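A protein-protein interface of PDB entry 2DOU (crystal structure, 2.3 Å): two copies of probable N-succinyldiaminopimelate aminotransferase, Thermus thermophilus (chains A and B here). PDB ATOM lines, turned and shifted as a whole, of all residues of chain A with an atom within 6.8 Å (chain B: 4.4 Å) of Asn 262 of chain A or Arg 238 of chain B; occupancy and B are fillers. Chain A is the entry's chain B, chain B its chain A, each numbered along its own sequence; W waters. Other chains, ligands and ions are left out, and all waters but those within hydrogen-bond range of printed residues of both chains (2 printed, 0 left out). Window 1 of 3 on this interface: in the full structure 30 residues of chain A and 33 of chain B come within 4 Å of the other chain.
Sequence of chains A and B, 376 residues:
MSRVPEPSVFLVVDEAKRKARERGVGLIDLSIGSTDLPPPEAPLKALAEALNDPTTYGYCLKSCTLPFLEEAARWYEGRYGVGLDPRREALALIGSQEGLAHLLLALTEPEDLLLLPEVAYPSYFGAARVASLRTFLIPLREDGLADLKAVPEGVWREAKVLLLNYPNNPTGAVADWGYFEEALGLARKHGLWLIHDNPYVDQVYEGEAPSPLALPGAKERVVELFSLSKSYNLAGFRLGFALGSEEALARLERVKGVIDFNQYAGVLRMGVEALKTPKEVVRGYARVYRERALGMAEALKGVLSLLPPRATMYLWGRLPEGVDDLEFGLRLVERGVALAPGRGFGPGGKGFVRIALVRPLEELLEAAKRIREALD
Gln 263 of chain B touches its own counterpart, Gln 263 of chain A.
Positions printed for both chains: 93, 94 and 263.
O of Gly 58 of chain A touches CA of Gly 236 of chain B, at 3.2 Å.
Tyr 59 of chain A touches Ala 235 of chain B.
NH1 of Arg 238 of chain B touches CE2 of Tyr 59 of chain A, at 3.3 Å.
Ile 259 of chain A touches Gln 97 of chain B (O to CG, 3.2 Å).
Phe 261 of chain A touches Gln 97 of chain B (CZ to NE2, 3.4 Å).
NH2 of Arg 238 of chain B touches CD1 of Phe 261 of chain A (3.4 Å).
O of Asn 262 of chain A touches CG of Arg 238 of chain B, at 3.5 Å.
CA of Tyr 264 of chain A touches O of Gly 236 of chain B (3.1 Å).
Phe 237 of chain B touches Tyr 264 of chain A.
Arg 238 of chain B touches just these residues of chain A: Tyr 59 (3.3 Å), Phe 261 (3.4 Å) and Asn 262 (3.5 Å).
Of the printed residues of chain B, Tyr 264 of chain A touches Gly 236 (3.1 Å) and Phe 237 (3.5 Å).
Printed residues of chain A within 4 Å of Gln 263 of chain B: Gln 263.
Leu 93 of chain B touches none of the printed residues of chain A.
Ser 63 of chain A touches none of the printed residues of chain B.
The nearest printed residue of chain A that does not touch Phe 237 of chain B is Gln 263 of chain A (4.7 Å).
Water W1 lies within hydrogen-bond range of the guanidinium group (NH2) of Arg 238 of chain B, the backbone carbonyl oxygen (O) of Ile 94 of chain B and the backbone carbonyl oxygen (O) of Ile 259 of chain A.
Water W2 lies within hydrogen-bond range of the guanidinium group (NE) of Arg 238 of chain B (2.7 Å), the backbone carbonyl oxygen (O) of Asn 262 of chain A (3.0 Å) and the backbone NH (N) of Phe 261 of chain A (3.0 Å).
The side-chain amide oxygen of Gln 263 of chain A lies within hydrogen-bond range of the side-chain amide nitrogen of Gln 263 of chain B, at 2.9 Å.
O of Ala 235 of chain B sits at hydrogen-bond distance from NH1 of Arg 238 of chain B, 3.0 Å away.
The backbone carbonyl oxygen (O) of Phe 237 of chain B is in hydrogen-bond range of the side-chain amide nitrogen (NE2) of Gln 263 of chain B (2.8 Å).
The backbone carbonyl oxygen of Cys 60 of chain A sits at hydrogen-bond distance from the side-chain amide nitrogen of Asn 262 of chain A (2.6 Å).
The backbone NH (N) of Asn 262 of chain A is in hydrogen-bond range of the side-chain carboxylate (OD1) of Asp 260 of chain A, 2.6 Å away.
SG of Cys 60 of chain A forms a disulfide with SG of Cys 64 of chain A (2.0 Å).
Of the 21 printed residues of chain A, 7 touch a printed residue of chain B.
Hydrophobic or aromatic side chains of chain A within 4 Å of the printed part of chain B: Tyr 59, Phe 261 and Tyr 264.
Of the 12 printed residues of chain B, 6 touch a printed residue of chain A.
Printed residues of chain B that touch a printed residue of chain A: Gln 97, Ala 235, Gly 236, Phe 237, Arg 238 and Gln 263.
Hydrophobic or aromatic side chains of chain B that line the printed part of chain A: Ala 235 and Phe 237.
Among the printed residues, no Asp or Glu carboxylate lies within 4 Å of a Lys or Arg side-chain nitrogen of the other chain.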
ATOM      1  N   GLY A  58      13.432   2.020  15.092  1.00  0.00           N
ATOM      2  CA  GLY A  58      13.851   3.403  14.940  1.00  0.00           C
ATOM      3  C   GLY A  58      14.782   3.775  16.082  1.00  0.00           C
ATOM      4  O   GLY A  58      15.094   2.933  16.919  1.00  0.00           O
ATOM      5  N   TYR A  59      15.230   5.026  16.129  1.00  0.00           N
ATOM      6  CA  TYR A  59      16.134   5.470  17.191  1.00  0.00           C
ATOM      7  C   TYR A  59      15.446   5.407  18.560  1.00  0.00           C
ATOM      8  O   TYR A  59      14.267   5.741  18.676  1.00  0.00           O
ATOM      9  CB  TYR A  59      16.576   6.912  16.953  1.00  0.00           C
ATOM     10  CG  TYR A  59      17.326   7.189  15.668  1.00  0.00           C
ATOM     11  CD1 TYR A  59      17.011   8.310  14.901  1.00  0.00           C
ATOM     12  CD2 TYR A  59      18.390   6.375  15.245  1.00  0.00           C
ATOM     13  CE1 TYR A  59      17.720   8.625  13.753  1.00  0.00           C
ATOM     14  CE2 TYR A  59      19.117   6.687  14.086  1.00  0.00           C
ATOM     15  CZ  TYR A  59      18.770   7.816  13.347  1.00  0.00           C
ATOM     16  OH  TYR A  59      19.436   8.138  12.192  1.00  0.00           O
ATOM     17  N   CYS A  60      16.177   4.963  19.582  1.00  0.00           N
ATOM     18  CA  CYS A  60      15.638   4.909  20.938  1.00  0.00           C
ATOM     19  C   CYS A  60      16.047   6.252  21.533  1.00  0.00           C
ATOM     20  O   CYS A  60      17.172   6.422  21.991  1.00  0.00           O
ATOM     21  CB  CYS A  60      16.251   3.748  21.750  1.00  0.00           C
ATOM     22  SG  CYS A  60      15.733   3.553  23.515  1.00  0.00           S
ATOM     23  N   LEU A  61      15.137   7.218  21.490  1.00  0.00           N
ATOM     24  CA  LEU A  61      15.425   8.541  22.031  1.00  0.00           C
ATOM     25  C   LEU A  61      15.272   8.586  23.555  1.00  0.00           C
ATOM     26  O   LEU A  61      14.944   7.574  24.185  1.00  0.00           O
ATOM     27  CB  LEU A  61      14.540   9.582  21.348  1.00  0.00           C
ATOM     28  CG  LEU A  61      15.017   9.892  19.922  1.00  0.00           C
ATOM     29  CD1 LEU A  61      13.895  10.512  19.107  1.00  0.00           C
ATOM     30  CD2 LEU A  61      16.221  10.822  19.979  1.00  0.00           C
ATOM     31  N   LYS A  62      15.527   9.758  24.135  1.00  0.00           N
ATOM     32  CA  LYS A  62      15.461   9.946  25.584  1.00  0.00           C
ATOM     33  C   LYS A  62      14.314   9.212  26.288  1.00  0.00           C
ATOM     34  O   LYS A  62      14.559   8.335  27.114  1.00  0.00           O
ATOM     35  CB  LYS A  62      15.409  11.447  25.914  1.00  0.00           C
ATOM     36  CG  LYS A  62      15.495  11.767  27.403  1.00  0.00           C
ATOM     37  CD  LYS A  62      16.762  11.189  28.029  1.00  0.00           C
ATOM     38  CE  LYS A  62      16.864  11.510  29.528  1.00  0.00           C
ATOM     39  NZ  LYS A  62      17.201  12.946  29.817  1.00  0.00           N
ATOM     40  N   SER A  63      13.072   9.550  25.954  1.00  0.00           N
ATOM     41  CA  SER A  63      11.935   8.910  26.604  1.00  0.00           C
ATOM     42  C   SER A  63      12.023   7.395  26.518  1.00  0.00           C
ATOM     43  O   SER A  63      11.653   6.697  27.465  1.00  0.00           O
ATOM     44  CB  SER A  63      10.612   9.390  25.996  1.00  0.00           C
ATOM     45  OG  SER A  63      10.369   8.777  24.742  1.00  0.00           O
ATOM     46  N   CYS A  64      12.516   6.892  25.384  1.00  0.00           N
ATOM     47  CA  CYS A  64      12.672   5.454  25.174  1.00  0.00           C
ATOM     48  C   CYS A  64      13.618   4.853  26.215  1.00  0.00           C
ATOM     49  O   CYS A  64      13.504   3.686  26.561  1.00  0.00           O
ATOM     50  CB  CYS A  64      13.180   5.171  23.741  1.00  0.00           C
ATOM     51  SG  CYS A  64      13.704   3.445  23.447  1.00  0.00           S
ATOM     52  N   THR A  65      14.539   5.657  26.734  1.00  0.00           N
ATOM     53  CA  THR A  65      15.466   5.165  27.743  1.00  0.00           C
ATOM     54  C   THR A  65      14.972   5.244  29.204  1.00  0.00           C
ATOM     55  O   THR A  65      15.621   4.693  30.097  1.00  0.00           O
ATOM     56  CB  THR A  65      16.845   5.893  27.659  1.00  0.00           C
ATOM     57  OG1 THR A  65      16.694   7.284  27.962  1.00  0.00           O
ATOM     58  CG2 THR A  65      17.436   5.761  26.258  1.00  0.00           C
ATOM     59  N   LEU A  91      21.437   9.364  32.868  1.00  0.00           N
ATOM     60  CA  LEU A  91      21.529   9.367  31.410  1.00  0.00           C
ATOM     61  C   LEU A  91      22.103   8.049  30.897  1.00  0.00           C
ATOM     62  O   LEU A  91      23.138   7.586  31.371  1.00  0.00           O
ATOM     63  CB  LEU A  91      22.403  10.527  30.917  1.00  0.00           C
ATOM     64  CG  LEU A  91      22.255  10.912  29.437  1.00  0.00           C
ATOM     65  CD1 LEU A  91      20.869  11.507  29.200  1.00  0.00           C
ATOM     66  CD2 LEU A  91      23.331  11.919  29.047  1.00  0.00           C
ATOM     67  N   ALA A  92      21.413   7.439  29.943  1.00  0.00           N
ATOM     68  CA  ALA A  92      21.865   6.187  29.348  1.00  0.00           C
ATOM     69  C   ALA A  92      23.167   6.433  28.593  1.00  0.00           C
ATOM     70  O   ALA A  92      23.321   7.448  27.917  1.00  0.00           O
ATOM     71  CB  ALA A  92      20.814   5.651  28.392  1.00  0.00           C
ATOM     72  N   LEU A  93      24.114   5.516  28.739  1.00  0.00           N
ATOM     73  CA  LEU A  93      25.393   5.623  28.041  1.00  0.00           C
ATOM     74  C   LEU A  93      25.564   4.390  27.138  1.00  0.00           C
ATOM     75  O   LEU A  93      25.119   3.295  27.490  1.00  0.00           O
ATOM     76  CB  LEU A  93      26.546   5.673  29.048  1.00  0.00           C
ATOM     77  CG  LEU A  93      26.488   6.707  30.179  1.00  0.00           C
ATOM     78  CD1 LEU A  93      27.710   6.530  31.071  1.00  0.00           C
ATOM     79  CD2 LEU A  93      26.444   8.116  29.609  1.00  0.00           C
ATOM     80  N   ILE A  94      26.192   4.571  25.976  1.00  0.00           N
ATOM     81  CA  ILE A  94      26.444   3.448  25.064  1.00  0.00           C
ATOM     82  C   ILE A  94      27.781   2.881  25.532  1.00  0.00           C
ATOM     83  O   ILE A  94      28.769   2.861  24.791  1.00  0.00           O
ATOM     84  CB  ILE A  94      26.576   3.920  23.597  1.00  0.00           C
ATOM     85  CG1 ILE A  94      25.384   4.810  23.228  1.00  0.00           C
ATOM     86  CG2 ILE A  94      26.622   2.710  22.662  1.00  0.00           C
ATOM     87  CD1 ILE A  94      25.556   5.550  21.917  1.00  0.00           C
ATOM     88  N   LYS A 256      26.188  14.370  23.669  1.00  0.00           N
ATOM     89  CA  LYS A 256      25.807  13.088  23.082  1.00  0.00           C
ATOM     90  C   LYS A 256      24.649  13.272  22.113  1.00  0.00           C
ATOM     91  O   LYS A 256      24.375  12.407  21.288  1.00  0.00           O
ATOM     92  CB  LYS A 256      25.402  12.084  24.164  1.00  0.00           C
ATOM     93  CG  LYS A 256      26.561  11.385  24.845  1.00  0.00           C
ATOM     94  CD  LYS A 256      26.088  10.537  26.025  1.00  0.00           C
ATOM     95  CE  LYS A 256      25.022   9.516  25.629  1.00  0.00           C
ATOM     96  NZ  LYS A 256      25.531   8.448  24.709  1.00  0.00           N
ATOM     97  N   ILE A 259      26.015  13.755  18.688  1.00  0.00           N
ATOM     98  CA  ILE A 259      26.948  12.692  18.363  1.00  0.00           C
ATOM     99  C   ILE A 259      26.299  11.329  18.162  1.00  0.00           C
ATOM    100  O   ILE A 259      26.647  10.615  17.223  1.00  0.00           O
ATOM    101  CB  ILE A 259      28.049  12.577  19.457  1.00  0.00           C
ATOM    102  CG1 ILE A 259      29.009  13.762  19.357  1.00  0.00           C
ATOM    103  CG2 ILE A 259      28.803  11.262  19.327  1.00  0.00           C
ATOM    104  CD1 ILE A 259      30.201  13.683  20.308  1.00  0.00           C
ATOM    105  N   ASP A 260      25.345  10.979  19.015  1.00  0.00           N
ATOM    106  CA  ASP A 260      24.698   9.677  18.919  1.00  0.00           C
ATOM    107  C   ASP A 260      23.177   9.715  19.099  1.00  0.00           C
ATOM    108  O   ASP A 260      22.582  10.784  19.201  1.00  0.00           O
ATOM    109  CB  ASP A 260      25.330   8.733  19.953  1.00  0.00           C
ATOM    110  CG  ASP A 260      24.886   9.037  21.397  1.00  0.00           C
ATOM    111  OD1 ASP A 260      23.690   8.844  21.697  1.00  0.00           O
ATOM    112  OD2 ASP A 260      25.735   9.451  22.219  1.00  0.00           O
ATOM    113  N   PHE A 261      22.559   8.536  19.093  1.00  0.00           N
ATOM    114  CA  PHE A 261      21.117   8.391  19.284  1.00  0.00           C
ATOM    115  C   PHE A 261      20.888   7.261  20.281  1.00  0.00           C
ATOM    116  O   PHE A 261      19.861   6.582  20.241  1.00  0.00           O
ATOM    117  CB  PHE A 261      20.390   8.039  17.981  1.00  0.00           C
ATOM    118  CG  PHE A 261      20.467   9.103  16.926  1.00  0.00           C
ATOM    119  CD1 PHE A 261      21.491   9.092  15.981  1.00  0.00           C
ATOM    120  CD2 PHE A 261      19.510  10.114  16.865  1.00  0.00           C
ATOM    121  CE1 PHE A 261      21.563  10.066  14.987  1.00  0.00           C
ATOM    122  CE2 PHE A 261      19.573  11.101  15.870  1.00  0.00           C
ATOM    123  CZ  PHE A 261      20.602  11.076  14.929  1.00  0.00           C
ATOM    124  N   ASN A 262      21.855   7.064  21.170  1.00  0.00           N
ATOM    125  CA  ASN A 262      21.765   6.015  22.179  1.00  0.00           C
ATOM    126  C   ASN A 262      21.901   4.632  21.546  1.00  0.00           C
ATOM    127  O   ASN A 262      22.130   4.505  20.342  1.00  0.00           O
ATOM    128  CB  ASN A 262      20.427   6.114  22.936  1.00  0.00           C
ATOM    129  CG  ASN A 262      20.134   7.527  23.411  1.00  0.00           C
ATOM    130  OD1 ASN A 262      20.963   8.145  24.072  1.00  0.00           O
ATOM    131  ND2 ASN A 262      18.954   8.045  23.067  1.00  0.00           N
ATOM    132  N   GLN A 263      21.750   3.600  22.365  1.00  0.00           N
ATOM    133  CA  GLN A 263      21.857   2.225  21.907  1.00  0.00           C
ATOM    134  C   GLN A 263      20.490   1.728  21.458  1.00  0.00           C
ATOM    135  O   GLN A 263      19.478   2.406  21.664  1.00  0.00           O
ATOM    136  CB  GLN A 263      22.398   1.350  23.040  1.00  0.00           C
ATOM    137  CG  GLN A 263      22.545  -0.127  22.713  1.00  0.00           C
ATOM    138  CD  GLN A 263      23.594  -0.380  21.647  1.00  0.00           C
ATOM    139  OE1 GLN A 263      23.387  -0.069  20.479  1.00  0.00           O
ATOM    140  NE2 GLN A 263      24.729  -0.924  22.052  1.00  0.00           N
ATOM    141  N   TYR A 264      20.471   0.551  20.837  1.00  0.00           N
ATOM    142  CA  TYR A 264      19.239  -0.070  20.357  1.00  0.00           C
ATOM    143  C   TYR A 264      18.273  -0.308  21.518  1.00  0.00           C
ATOM    144  O   TYR A 264      18.686  -0.785  22.577  1.00  0.00           O
ATOM    145  CB  TYR A 264      19.570  -1.402  19.670  1.00  0.00           C
ATOM    146  CG  TYR A 264      18.389  -2.319  19.415  1.00  0.00           C
ATOM    147  CD1 TYR A 264      17.276  -1.881  18.703  1.00  0.00           C
ATOM    148  CD2 TYR A 264      18.404  -3.637  19.860  1.00  0.00           C
ATOM    149  CE1 TYR A 264      16.209  -2.732  18.439  1.00  0.00           C
ATOM    150  CE2 TYR A 264      17.341  -4.500  19.598  1.00  0.00           C
ATOM    151  CZ  TYR A 264      16.249  -4.040  18.892  1.00  0.00           C
ATOM    152  OH  TYR A 264      15.193  -4.881  18.652  1.00  0.00           O
ATOM    153  N   ALA A 265      16.998   0.019  21.296  1.00  0.00           N
ATOM    154  CA  ALA A 265      15.949  -0.145  22.307  1.00  0.00           C
ATOM    155  C   ALA A 265      15.992  -1.539  22.930  1.00  0.00           C
ATOM    156  O   ALA A 265      15.826  -1.691  24.148  1.00  0.00           O
ATOM    157  CB  ALA A 265      14.573   0.109  21.688  1.00  0.00           C
ATOM    158  N   LEU A 268      18.317  -1.624  25.693  1.00  0.00           N
ATOM    159  CA  LEU A 268      17.878  -0.895  26.879  1.00  0.00           C
ATOM    160  C   LEU A 268      17.005  -1.827  27.721  1.00  0.00           C
ATOM    161  O   LEU A 268      17.113  -1.855  28.954  1.00  0.00           O
ATOM    162  CB  LEU A 268      17.100   0.369  26.483  1.00  0.00           C
ATOM    163  CG  LEU A 268      17.917   1.638  26.213  1.00  0.00           C
ATOM    164  CD1 LEU A 268      18.536   2.119  27.505  1.00  0.00           C
ATOM    165  CD2 LEU A 268      19.010   1.383  25.173  1.00  0.00           C
ATOM    166  N   LEU B  93      31.359   2.005  12.086  1.00  0.00           N
ATOM    167  CA  LEU B  93      30.851   3.143  12.839  1.00  0.00           C
ATOM    168  C   LEU B  93      29.620   2.705  13.616  1.00  0.00           C
ATOM    169  O   LEU B  93      28.862   1.850  13.146  1.00  0.00           O
ATOM    170  CB  LEU B  93      30.461   4.287  11.888  1.00  0.00           C
ATOM    171  CG  LEU B  93      31.515   4.733  10.865  1.00  0.00           C
ATOM    172  CD1 LEU B  93      30.954   5.826   9.966  1.00  0.00           C
ATOM    173  CD2 LEU B  93      32.755   5.230  11.596  1.00  0.00           C
ATOM    174  N   ILE B  94      29.428   3.282  14.805  1.00  0.00           N
ATOM    175  CA  ILE B  94      28.256   2.968  15.613  1.00  0.00           C
ATOM    176  C   ILE B  94      27.196   3.972  15.161  1.00  0.00           C
ATOM    177  O   ILE B  94      26.702   4.784  15.953  1.00  0.00           O
ATOM    178  CB  ILE B  94      28.534   3.169  17.115  1.00  0.00           C
ATOM    179  CG1 ILE B  94      29.852   2.501  17.495  1.00  0.00           C
ATOM    180  CG2 ILE B  94      27.423   2.551  17.925  1.00  0.00           C
ATOM    181  CD1 ILE B  94      30.289   2.767  18.910  1.00  0.00           C
ATOM    182  N   GLY B  95      26.847   3.891  13.876  1.00  0.00           N
ATOM    183  CA  GLY B  95      25.901   4.815  13.273  1.00  0.00           C
ATOM    184  C   GLY B  95      26.792   5.897  12.688  1.00  0.00           C
ATOM    185  O   GLY B  95      27.865   6.139  13.228  1.00  0.00           O
ATOM    186  N   GLN B  97      26.346   9.268  12.517  1.00  0.00           N
ATOM    187  CA  GLN B  97      26.386  10.489  13.328  1.00  0.00           C
ATOM    188  C   GLN B  97      27.664  10.508  14.152  1.00  0.00           C
ATOM    189  O   GLN B  97      28.401  11.488  14.196  1.00  0.00           O
ATOM    190  CB  GLN B  97      25.192  10.519  14.276  1.00  0.00           C
ATOM    191  CG  GLN B  97      24.924  11.887  14.824  1.00  0.00           C
ATOM    192  CD  GLN B  97      24.202  12.738  13.816  1.00  0.00           C
ATOM    193  OE1 GLN B  97      24.633  12.863  12.658  1.00  0.00           O
ATOM    194  NE2 GLN B  97      23.087  13.332  14.239  1.00  0.00           N
ATOM    195  N   SER B 229      21.085   2.768   8.516  1.00  0.00           N
ATOM    196  CA  SER B 229      19.828   3.375   8.974  1.00  0.00           C
ATOM    197  C   SER B 229      18.774   3.666   7.917  1.00  0.00           C
ATOM    198  O   SER B 229      17.641   3.218   8.028  1.00  0.00           O
ATOM    199  CB  SER B 229      20.123   4.664   9.758  1.00  0.00           C
ATOM    200  OG  SER B 229      20.870   4.376  10.927  1.00  0.00           O
ATOM    201  N   LEU B 234      17.104   0.433   9.590  1.00  0.00           N
ATOM    202  CA  LEU B 234      17.653  -0.184  10.789  1.00  0.00           C
ATOM    203  C   LEU B 234      18.329   0.879  11.651  1.00  0.00           C
ATOM    204  O   LEU B 234      19.342   0.613  12.305  1.00  0.00           O
ATOM    205  CB  LEU B 234      18.672  -1.256  10.397  1.00  0.00           C
ATOM    206  CG  LEU B 234      18.121  -2.465   9.646  1.00  0.00           C
ATOM    207  CD1 LEU B 234      19.279  -3.355   9.237  1.00  0.00           C
ATOM    208  CD2 LEU B 234      17.137  -3.229  10.523  1.00  0.00           C
ATOM    209  N   ALA B 235      17.760   2.082  11.638  1.00  0.00           N
ATOM    210  CA  ALA B 235      18.300   3.211  12.400  1.00  0.00           C
ATOM    211  C   ALA B 235      18.611   2.874  13.858  1.00  0.00           C
ATOM    212  O   ALA B 235      19.668   3.233  14.374  1.00  0.00           O
ATOM    213  CB  ALA B 235      17.336   4.397  12.328  1.00  0.00           C
ATOM    214  N   GLY B 236      17.702   2.158  14.505  1.00  0.00           N
ATOM    215  CA  GLY B 236      17.903   1.808  15.895  1.00  0.00           C
ATOM    216  C   GLY B 236      19.071   0.902  16.233  1.00  0.00           C
ATOM    217  O   GLY B 236      19.524   0.886  17.383  1.00  0.00           O
ATOM    218  N   PHE B 237      19.579   0.155  15.256  1.00  0.00           N
ATOM    219  CA  PHE B 237      20.679  -0.763  15.531  1.00  0.00           C
ATOM    220  C   PHE B 237      22.060  -0.130  15.503  1.00  0.00           C
ATOM    221  O   PHE B 237      23.056  -0.767  15.840  1.00  0.00           O
ATOM    222  CB  PHE B 237      20.585  -1.974  14.600  1.00  0.00           C
ATOM    223  CG  PHE B 237      19.286  -2.720  14.731  1.00  0.00           C
ATOM    224  CD1 PHE B 237      18.164  -2.320  14.017  1.00  0.00           C
ATOM    225  CD2 PHE B 237      19.165  -3.775  15.624  1.00  0.00           C
ATOM    226  CE1 PHE B 237      16.936  -2.960  14.191  1.00  0.00           C
ATOM    227  CE2 PHE B 237      17.944  -4.420  15.806  1.00  0.00           C
ATOM    228  CZ  PHE B 237      16.827  -4.011  15.088  1.00  0.00           C
ATOM    229  N   ARG B 238      22.108   1.132  15.104  1.00  0.00           N
ATOM    230  CA  ARG B 238      23.342   1.904  15.098  1.00  0.00           C
ATOM    231  C   ARG B 238      24.560   1.267  14.417  1.00  0.00           C
ATOM    232  O   ARG B 238      25.498   0.826  15.082  1.00  0.00           O
ATOM    233  CB  ARG B 238      23.722   2.266  16.543  1.00  0.00           C
ATOM    234  CG  ARG B 238      22.544   2.675  17.446  1.00  0.00           C
ATOM    235  CD  ARG B 238      21.777   3.848  16.866  1.00  0.00           C
ATOM    236  NE  ARG B 238      22.670   4.964  16.582  1.00  0.00           N
ATOM    237  CZ  ARG B 238      22.759   5.568  15.404  1.00  0.00           C
ATOM    238  NH1 ARG B 238      22.007   5.168  14.391  1.00  0.00           N
ATOM    239  NH2 ARG B 238      23.607   6.569  15.239  1.00  0.00           N
ATOM    240  N   LEU B 239      24.550   1.225  13.093  1.00  0.00           N
ATOM    241  CA  LEU B 239      25.689   0.681  12.371  1.00  0.00           C
ATOM    242  C   LEU B 239      25.883   1.423  11.063  1.00  0.00           C
ATOM    243  O   LEU B 239      24.936   1.655  10.317  1.00  0.00           O
ATOM    244  CB  LEU B 239      25.511  -0.815  12.092  1.00  0.00           C
ATOM    245  CG  LEU B 239      26.754  -1.502  11.506  1.00  0.00           C
ATOM    246  CD1 LEU B 239      27.886  -1.470  12.528  1.00  0.00           C
ATOM    247  CD2 LEU B 239      26.428  -2.936  11.126  1.00  0.00           C
ATOM    248  N   GLN B 263      30.212  -1.495  17.886  1.00  0.00           N
ATOM    249  CA  GLN B 263      28.912  -2.044  18.215  1.00  0.00           C
ATOM    250  C   GLN B 263      29.009  -3.539  18.548  1.00  0.00           C
ATOM    251  O   GLN B 263      30.061  -4.166  18.384  1.00  0.00           O
ATOM    252  CB  GLN B 263      27.960  -1.803  17.041  1.00  0.00           C
ATOM    253  CG  GLN B 263      26.546  -2.271  17.245  1.00  0.00           C
ATOM    254  CD  GLN B 263      25.840  -1.540  18.380  1.00  0.00           C
ATOM    255  OE1 GLN B 263      26.292  -1.562  19.518  1.00  0.00           O
ATOM    256  NE2 GLN B 263      24.727  -0.899  18.065  1.00  0.00           N
HETATM  257  O   HOH W   1      25.995   7.464  15.949  1.00  0.00           O
HETATM  258  O   HOH W   2      24.057   5.976  18.613  1.00  0.00           O
